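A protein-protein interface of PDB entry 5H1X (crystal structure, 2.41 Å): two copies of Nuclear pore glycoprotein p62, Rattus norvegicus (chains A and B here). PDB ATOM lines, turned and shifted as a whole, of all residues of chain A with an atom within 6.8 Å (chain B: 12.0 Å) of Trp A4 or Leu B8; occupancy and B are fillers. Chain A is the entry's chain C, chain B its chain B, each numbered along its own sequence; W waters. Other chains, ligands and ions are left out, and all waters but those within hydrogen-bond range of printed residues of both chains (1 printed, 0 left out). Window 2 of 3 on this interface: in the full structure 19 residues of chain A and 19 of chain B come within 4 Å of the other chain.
NE1 of Trp A4 sits at hydrogen-bond distance from OD1 of Asp B5, at 3.0 Å.
The backbone NH of Gly B12 lies close to the side-chain amide nitrogen of Asn A11, 3.3 Å away.
The backbone carbonyl oxygen (O) of Thr B7 sits close to the side-chain amide oxygen (OD1) of Asn B11 (3.1 Å).
The backbone carbonyl oxygen (O) of Gly B12 lies within hydrogen-bond range of the side-chain hydroxyl (OG1) of Thr B16, at 2.9 Å.
The side-chain amide nitrogen of Asn A2 sits close to the backbone NH of Trp A4.
OG1 of Thr A7 lies within hydrogen-bond range of O of Ala A3 (2.9 Å).
The side-chain amide oxygen of Asn A11 lies close to the backbone carbonyl oxygen of Thr A7, at 3.2 Å.
Of the 9 printed residues of chain A, 4 touch a printed residue of chain B.
Along chain A the printed residues that touch a printed residue of chain B span positions 4 to 11.
Printed residues of chain B that touch a printed residue of chain A: Asp B5, Leu B8, Asn B11 and Gly B12.
Among the printed residues, 7 pairs touch across the chains.
Leu B8 touches just these residues of chain A: Trp A4 (3.9 Å), Thr A7 (3.8 Å), Leu A8 (3.7 Å) and Asn A11 (3.6 Å).
No residue of chain B comes within 4 Å of Asn A2.
Ala A3 touches none of the printed residues of chain B.
Thr A7 touches one residue of chain B.
Of chain B, only Leu B8 comes within 4 Å of Leu A8.
Printed residues of chain A within 4 Å of Gly B12: Asn A11.
Printed residues of chain B within 4 Å of Asn A11: Leu B8, Asn B11 and Gly B12.
Of the printed residues of chain A, Asp B5 touches Trp A4.
Of the printed residues of chain A, Asn B11 touches Asn A11.
Thr B16 touches none of the printed residues of chain A.
Water W1 lies within hydrogen-bond range of the side-chain amide nitrogen (ND2) of Asn B11 and the side-chain amide nitrogen (ND2) of Asn A11.
O of Trp A4 touches CD2 of Leu B8 (3.9 Å).
CG2 of Thr A7 touches CG of Leu B8 (3.8 Å).
CD1 of Leu B8 touches CD1 of Leu A8 (3.7 Å).
Asn A11 touches Leu B8 (ND2 to O, 3.6 Å).
Asn A11 touches Asn B11 (ND2 to CB, 3.5 Å).
Trp A4 touches Asp B5, but with the chains exchanged Asp A5 does not touch Trp B4 (10.1 Å).
Trp A4 touches Leu B8, but with the chains exchanged Leu A8 does not touch Trp B4 (7.7 Å).
Thr A7 touches Leu B8, but with the chains exchanged Leu A8 does not touch Thr B7 (7.6 Å).
Leu B8 touches its own counterpart, Leu A8.
Of the 7 pairs that touch across the chains among the printed residues, 2 have their exchanged pair printed and touching as well.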
ATOM      1  N   ASN A   2      15.651  26.004  -3.539  1.00  0.00           N
ATOM      2  CA  ASN A   2      14.922  24.984  -2.794  1.00  0.00           C
ATOM      3  C   ASN A   2      15.870  24.125  -1.963  1.00  0.00           C
ATOM      4  O   ASN A   2      17.082  24.187  -2.149  1.00  0.00           O
ATOM      5  CB  ASN A   2      14.141  24.096  -3.750  1.00  0.00           C
ATOM      6  CG  ASN A   2      15.047  23.422  -4.742  1.00  0.00           C
ATOM      7  OD1 ASN A   2      15.760  24.091  -5.484  1.00  0.00           O
ATOM      8  ND2 ASN A   2      15.077  22.101  -4.720  1.00  0.00           N
ATOM      9  N   ALA A   3      15.319  23.306  -1.073  1.00  0.00           N
ATOM     10  CA  ALA A   3      16.131  22.514  -0.149  1.00  0.00           C
ATOM     11  C   ALA A   3      17.021  21.464  -0.832  1.00  0.00           C
ATOM     12  O   ALA A   3      18.100  21.149  -0.327  1.00  0.00           O
ATOM     13  CB  ALA A   3      15.240  21.842   0.859  1.00  0.00           C
ATOM     14  N   TRP A   4      16.571  20.918  -1.964  1.00  0.00           N
ATOM     15  CA  TRP A   4      17.337  19.880  -2.655  1.00  0.00           C
ATOM     16  C   TRP A   4      18.634  20.432  -3.275  1.00  0.00           C
ATOM     17  O   TRP A   4      19.735  19.936  -2.975  1.00  0.00           O
ATOM     18  CB  TRP A   4      16.484  19.203  -3.721  1.00  0.00           C
ATOM     19  CG  TRP A   4      15.313  18.444  -3.158  1.00  0.00           C
ATOM     20  CD1 TRP A   4      15.317  17.166  -2.676  1.00  0.00           C
ATOM     21  CD2 TRP A   4      13.957  18.914  -3.030  1.00  0.00           C
ATOM     22  NE1 TRP A   4      14.053  16.818  -2.247  1.00  0.00           N
ATOM     23  CE2 TRP A   4      13.206  17.875  -2.455  1.00  0.00           C
ATOM     24  CE3 TRP A   4      13.319  20.119  -3.346  1.00  0.00           C
ATOM     25  CZ2 TRP A   4      11.844  17.999  -2.185  1.00  0.00           C
ATOM     26  CZ3 TRP A   4      11.964  20.239  -3.081  1.00  0.00           C
ATOM     27  CH2 TRP A   4      11.243  19.185  -2.505  1.00  0.00           C
ATOM     28  N   ASP A   5      18.514  21.462  -4.115  1.00  0.00           N
ATOM     29  CA  ASP A   5      19.690  22.036  -4.771  1.00  0.00           C
ATOM     30  C   ASP A   5      20.650  22.675  -3.757  1.00  0.00           C
ATOM     31  O   ASP A   5      21.859  22.756  -3.996  1.00  0.00           O
ATOM     32  CB  ASP A   5      19.298  23.079  -5.844  1.00  0.00           C
ATOM     33  CG  ASP A   5      18.092  22.645  -6.737  1.00  0.00           C
ATOM     34  OD1 ASP A   5      17.903  21.444  -6.998  1.00  0.00           O
ATOM     35  OD2 ASP A   5      17.382  23.520  -7.271  1.00  0.00           O
ATOM     36  N   ARG A   6      20.112  23.139  -2.635  1.00  0.00           N
ATOM     37  CA  ARG A   6      20.934  23.726  -1.597  1.00  0.00           C
ATOM     38  C   ARG A   6      21.831  22.652  -0.994  1.00  0.00           C
ATOM     39  O   ARG A   6      23.039  22.826  -0.885  1.00  0.00           O
ATOM     40  CB  ARG A   6      20.064  24.374  -0.520  1.00  0.00           C
ATOM     41  CG  ARG A   6      19.586  25.769  -0.915  1.00  0.00           C
ATOM     42  CD  ARG A   6      18.396  26.287  -0.099  1.00  0.00           C
ATOM     43  NE  ARG A   6      18.274  27.745  -0.206  1.00  0.00           N
ATOM     44  CZ  ARG A   6      17.341  28.390  -0.907  1.00  0.00           C
ATOM     45  NH1 ARG A   6      16.407  27.721  -1.563  1.00  0.00           N
ATOM     46  NH2 ARG A   6      17.335  29.719  -0.935  1.00  0.00           N
ATOM     47  N   THR A   7      21.225  21.539  -0.605  1.00  0.00           N
ATOM     48  CA  THR A   7      21.967  20.414  -0.083  1.00  0.00           C
ATOM     49  C   THR A   7      22.976  19.904  -1.112  1.00  0.00           C
ATOM     50  O   THR A   7      24.136  19.653  -0.782  1.00  0.00           O
ATOM     51  CB  THR A   7      21.013  19.290   0.324  1.00  0.00           C
ATOM     52  OG1 THR A   7      20.108  19.784   1.318  1.00  0.00           O
ATOM     53  CG2 THR A   7      21.776  18.113   0.883  1.00  0.00           C
ATOM     54  N   LEU A   8      22.542  19.773  -2.364  1.00  0.00           N
ATOM     55  CA  LEU A   8      23.414  19.233  -3.402  1.00  0.00           C
ATOM     56  C   LEU A   8      24.594  20.162  -3.699  1.00  0.00           C
ATOM     57  O   LEU A   8      25.702  19.694  -3.987  1.00  0.00           O
ATOM     58  CB  LEU A   8      22.622  18.957  -4.681  1.00  0.00           C
ATOM     59  CG  LEU A   8      23.292  18.140  -5.794  1.00  0.00           C
ATOM     60  CD1 LEU A   8      23.566  16.710  -5.358  1.00  0.00           C
ATOM     61  CD2 LEU A   8      22.406  18.144  -7.035  1.00  0.00           C
ATOM     62  N   ILE A   9      24.371  21.469  -3.620  1.00  0.00           N
ATOM     63  CA  ILE A   9      25.461  22.414  -3.824  1.00  0.00           C
ATOM     64  C   ILE A   9      26.454  22.440  -2.631  1.00  0.00           C
ATOM     65  O   ILE A   9      27.671  22.417  -2.853  1.00  0.00           O
ATOM     66  CB  ILE A   9      24.932  23.836  -4.092  1.00  0.00           C
ATOM     67  CG1 ILE A   9      24.395  23.928  -5.524  1.00  0.00           C
ATOM     68  CG2 ILE A   9      26.033  24.859  -3.922  1.00  0.00           C
ATOM     69  CD1 ILE A   9      23.517  25.146  -5.791  1.00  0.00           C
ATOM     70  N   ASN A  11      26.978  20.154  -0.274  1.00  0.00           N
ATOM     71  CA  ASN A  11      27.687  18.888  -0.272  1.00  0.00           C
ATOM     72  C   ASN A  11      28.902  18.936  -1.191  1.00  0.00           C
ATOM     73  O   ASN A  11      29.994  18.531  -0.795  1.00  0.00           O
ATOM     74  CB  ASN A  11      26.762  17.749  -0.670  1.00  0.00           C
ATOM     75  CG  ASN A  11      25.862  17.326   0.463  1.00  0.00           C
ATOM     76  OD1 ASN A  11      25.732  18.028   1.459  1.00  0.00           O
ATOM     77  ND2 ASN A  11      25.263  16.157   0.334  1.00  0.00           N
ATOM     78  N   ASN B   2      12.414   8.646  -3.775  1.00  0.00           N
ATOM     79  CA  ASN B   2      12.845   8.406  -2.400  1.00  0.00           C
ATOM     80  C   ASN B   2      14.332   8.043  -2.283  1.00  0.00           C
ATOM     81  O   ASN B   2      14.999   8.453  -1.344  1.00  0.00           O
ATOM     82  CB  ASN B   2      11.998   7.302  -1.769  1.00  0.00           C
ATOM     83  CG  ASN B   2      11.992   7.362  -0.269  1.00  0.00           C
ATOM     84  OD1 ASN B   2      12.979   7.032   0.369  1.00  0.00           O
ATOM     85  ND2 ASN B   2      10.867   7.771   0.312  1.00  0.00           N
ATOM     86  N   ALA B   3      14.846   7.280  -3.237  1.00  0.00           N
ATOM     87  CA  ALA B   3      16.268   6.905  -3.226  1.00  0.00           C
ATOM     88  C   ALA B   3      17.160   8.115  -3.450  1.00  0.00           C
ATOM     89  O   ALA B   3      18.234   8.204  -2.874  1.00  0.00           O
ATOM     90  CB  ALA B   3      16.551   5.852  -4.278  1.00  0.00           C
ATOM     91  N   TRP B   4      16.718   9.037  -4.303  1.00  0.00           N
ATOM     92  CA  TRP B   4      17.439  10.284  -4.536  1.00  0.00           C
ATOM     93  C   TRP B   4      17.502  11.102  -3.247  1.00  0.00           C
ATOM     94  O   TRP B   4      18.587  11.460  -2.783  1.00  0.00           O
ATOM     95  CB  TRP B   4      16.773  11.106  -5.642  1.00  0.00           C
ATOM     96  CG  TRP B   4      16.633  10.398  -6.980  1.00  0.00           C
ATOM     97  CD1 TRP B   4      17.586  10.287  -7.948  1.00  0.00           C
ATOM     98  CD2 TRP B   4      15.469   9.734  -7.485  1.00  0.00           C
ATOM     99  NE1 TRP B   4      17.091   9.593  -9.024  1.00  0.00           N
ATOM    100  CE2 TRP B   4      15.792   9.243  -8.769  1.00  0.00           C
ATOM    101  CE3 TRP B   4      14.185   9.511  -6.988  1.00  0.00           C
ATOM    102  CZ2 TRP B   4      14.873   8.541  -9.561  1.00  0.00           C
ATOM    103  CZ3 TRP B   4      13.274   8.817  -7.769  1.00  0.00           C
ATOM    104  CH2 TRP B   4      13.626   8.334  -9.041  1.00  0.00           C
ATOM    105  N   ASP B   5      16.336  11.377  -2.660  1.00  0.00           N
ATOM    106  CA  ASP B   5      16.253  12.127  -1.395  1.00  0.00           C
ATOM    107  C   ASP B   5      17.095  11.538  -0.286  1.00  0.00           C
ATOM    108  O   ASP B   5      17.688  12.263   0.523  1.00  0.00           O
ATOM    109  CB  ASP B   5      14.818  12.191  -0.899  1.00  0.00           C
ATOM    110  CG  ASP B   5      13.945  13.020  -1.788  1.00  0.00           C
ATOM    111  OD1 ASP B   5      14.496  13.899  -2.492  1.00  0.00           O
ATOM    112  OD2 ASP B   5      12.719  12.776  -1.788  1.00  0.00           O
ATOM    113  N   ARG B   6      17.125  10.216  -0.231  1.00  0.00           N
ATOM    114  CA  ARG B   6      17.751   9.551   0.885  1.00  0.00           C
ATOM    115  C   ARG B   6      19.261   9.497   0.685  1.00  0.00           C
ATOM    116  O   ARG B   6      20.008   9.540   1.642  1.00  0.00           O
ATOM    117  CB  ARG B   6      17.145   8.168   1.060  1.00  0.00           C
ATOM    118  CG  ARG B   6      18.092   7.080   1.501  1.00  0.00           C
ATOM    119  CD  ARG B   6      17.262   5.833   1.730  1.00  0.00           C
ATOM    120  NE  ARG B   6      17.983   4.757   2.401  1.00  0.00           N
ATOM    121  CZ  ARG B   6      17.365   3.748   3.004  1.00  0.00           C
ATOM    122  NH1 ARG B   6      16.035   3.726   3.022  1.00  0.00           N
ATOM    123  NH2 ARG B   6      18.058   2.784   3.599  1.00  0.00           N
ATOM    124  N   THR B   7      19.698   9.446  -0.567  1.00  0.00           N
ATOM    125  CA  THR B   7      21.113   9.538  -0.882  1.00  0.00           C
ATOM    126  C   THR B   7      21.621  10.958  -0.632  1.00  0.00           C
ATOM    127  O   THR B   7      22.776  11.153  -0.237  1.00  0.00           O
ATOM    128  CB  THR B   7      21.406   9.122  -2.354  1.00  0.00           C
ATOM    129  OG1 THR B   7      21.078   7.740  -2.537  1.00  0.00           O
ATOM    130  CG2 THR B   7      22.880   9.320  -2.700  1.00  0.00           C
ATOM    131  N   LEU B   8      20.760  11.946  -0.854  1.00  0.00           N
ATOM    132  CA  LEU B   8      21.132  13.345  -0.634  1.00  0.00           C
ATOM    133  C   LEU B   8      21.372  13.577   0.867  1.00  0.00           C
ATOM    134  O   LEU B   8      22.374  14.183   1.290  1.00  0.00           O
ATOM    135  CB  LEU B   8      20.047  14.268  -1.177  1.00  0.00           C
ATOM    136  CG  LEU B   8      20.311  15.711  -1.629  1.00  0.00           C
ATOM    137  CD1 LEU B   8      21.670  15.912  -2.264  1.00  0.00           C
ATOM    138  CD2 LEU B   8      19.226  16.137  -2.607  1.00  0.00           C
ATOM    139  N   ILE B   9      20.462  13.045   1.674  1.00  0.00           N
ATOM    140  CA  ILE B   9      20.566  13.153   3.118  1.00  0.00           C
ATOM    141  C   ILE B   9      21.779  12.403   3.688  1.00  0.00           C
ATOM    142  O   ILE B   9      22.550  12.966   4.459  1.00  0.00           O
ATOM    143  CB  ILE B   9      19.289  12.637   3.786  1.00  0.00           C
ATOM    144  CG1 ILE B   9      18.110  13.554   3.435  1.00  0.00           C
ATOM    145  CG2 ILE B   9      19.473  12.562   5.293  1.00  0.00           C
ATOM    146  CD1 ILE B   9      16.788  13.142   4.066  1.00  0.00           C
ATOM    147  N   GLU B  10      21.939  11.135   3.322  1.00  0.00           N
ATOM    148  CA  GLU B  10      23.043  10.335   3.836  1.00  0.00           C
ATOM    149  C   GLU B  10      24.383  10.959   3.431  1.00  0.00           C
ATOM    150  O   GLU B  10      25.292  11.062   4.254  1.00  0.00           O
ATOM    151  CB  GLU B  10      22.947   8.889   3.345  1.00  0.00           C
ATOM    152  CG  GLU B  10      21.763   8.120   3.915  1.00  0.00           C
ATOM    153  CD  GLU B  10      22.158   6.876   4.705  1.00  0.00           C
ATOM    154  OE1 GLU B  10      23.364   6.707   5.015  1.00  0.00           O
ATOM    155  OE2 GLU B  10      21.255   6.066   5.024  1.00  0.00           O
ATOM    156  N   ASN B  11      24.495  11.396   2.176  1.00  0.00           N
ATOM    157  CA  ASN B  11      25.654  12.184   1.760  1.00  0.00           C
ATOM    158  C   ASN B  11      25.941  13.362   2.691  1.00  0.00           C
ATOM    159  O   ASN B  11      27.072  13.535   3.163  1.00  0.00           O
ATOM    160  CB  ASN B  11      25.474  12.699   0.339  1.00  0.00           C
ATOM    161  CG  ASN B  11      25.822  11.657  -0.694  1.00  0.00           C
ATOM    162  OD1 ASN B  11      25.819  10.464  -0.400  1.00  0.00           O
ATOM    163  ND2 ASN B  11      26.166  12.099  -1.898  1.00  0.00           N
ATOM    164  N   GLY B  12      24.909  14.164   2.947  1.00  0.00           N
ATOM    165  CA  GLY B  12      25.020  15.311   3.832  1.00  0.00           C
ATOM    166  C   GLY B  12      25.393  14.950   5.258  1.00  0.00           C
ATOM    167  O   GLY B  12      26.204  15.637   5.882  1.00  0.00           O
ATOM    168  N   GLU B  13      24.789  13.883   5.775  1.00  0.00           N
ATOM    169  CA  GLU B  13      25.121  13.362   7.095  1.00  0.00           C
ATOM    170  C   GLU B  13      26.595  12.929   7.177  1.00  0.00           C
ATOM    171  O   GLU B  13      27.297  13.241   8.134  1.00  0.00           O
ATOM    172  CB  GLU B  13      24.208  12.175   7.430  1.00  0.00           C
ATOM    173  CG  GLU B  13      24.181  11.756   8.894  1.00  0.00           C
ATOM    174  CD  GLU B  13      25.391  10.955   9.318  1.00  0.00           C
ATOM    175  OE1 GLU B  13      26.151  10.500   8.433  1.00  0.00           O
ATOM    176  OE2 GLU B  13      25.586  10.775  10.544  1.00  0.00           O
ATOM    177  N   LYS B  14      27.032  12.184   6.167  1.00  0.00           N
ATOM    178  CA  LYS B  14      28.366  11.597   6.113  1.00  0.00           C
ATOM    179  C   LYS B  14      29.452  12.675   6.047  1.00  0.00           C
ATOM    180  O   LYS B  14      30.319  12.728   6.918  1.00  0.00           O
ATOM    181  CB  LYS B  14      28.459  10.645   4.914  1.00  0.00           C
ATOM    182  CG  LYS B  14      29.553   9.614   4.982  1.00  0.00           C
ATOM    183  CD  LYS B  14      29.320   8.450   4.025  1.00  0.00           C
ATOM    184  CE  LYS B  14      28.045   7.668   4.329  1.00  0.00           C
ATOM    185  NZ  LYS B  14      27.786   6.603   3.285  1.00  0.00           N
ATOM    186  N   ILE B  15      29.388  13.549   5.045  1.00  0.00           N
ATOM    187  CA  ILE B  15      30.382  14.615   4.869  1.00  0.00           C
ATOM    188  C   ILE B  15      30.453  15.532   6.110  1.00  0.00           C
ATOM    189  O   ILE B  15      31.519  16.048   6.478  1.00  0.00           O
ATOM    190  CB  ILE B  15      30.076  15.452   3.594  1.00  0.00           C
ATOM    191  CG1 ILE B  15      31.175  16.470   3.298  1.00  0.00           C
ATOM    192  CG2 ILE B  15      28.714  16.151   3.692  1.00  0.00           C
ATOM    193  CD1 ILE B  15      32.396  15.871   2.660  1.00  0.00           C
ATOM    194  N   THR B  16      29.321  15.704   6.779  1.00  0.00           N
ATOM    195  CA  THR B  16      29.296  16.493   7.997  1.00  0.00           C
ATOM    196  C   THR B  16      30.038  15.767   9.106  1.00  0.00           C
ATOM    197  O   THR B  16      30.806  16.376   9.836  1.00  0.00           O
ATOM    198  CB  THR B  16      27.860  16.802   8.419  1.00  0.00           C
ATOM    199  OG1 THR B  16      27.306  17.744   7.489  1.00  0.00           O
ATOM    200  CG2 THR B  16      27.818  17.383   9.829  1.00  0.00           C
ATOM    201  N   SER B  17      29.821  14.459   9.198  1.00  0.00           N
ATOM    202  CA  SER B  17      30.500  13.608  10.176  1.00  0.00           C
ATOM    203  C   SER B  17      31.984  13.460   9.884  1.00  0.00           C
ATOM    204  O   SER B  17      32.763  13.118  10.760  1.00  0.00           O
ATOM    205  CB  SER B  17      29.852  12.228  10.219  1.00  0.00           C
ATOM    206  OG  SER B  17      30.614  11.323  10.986  1.00  0.00           O
HETATM  207  O   HOH W   1      25.419  15.006  -2.774  1.00  0.00           O
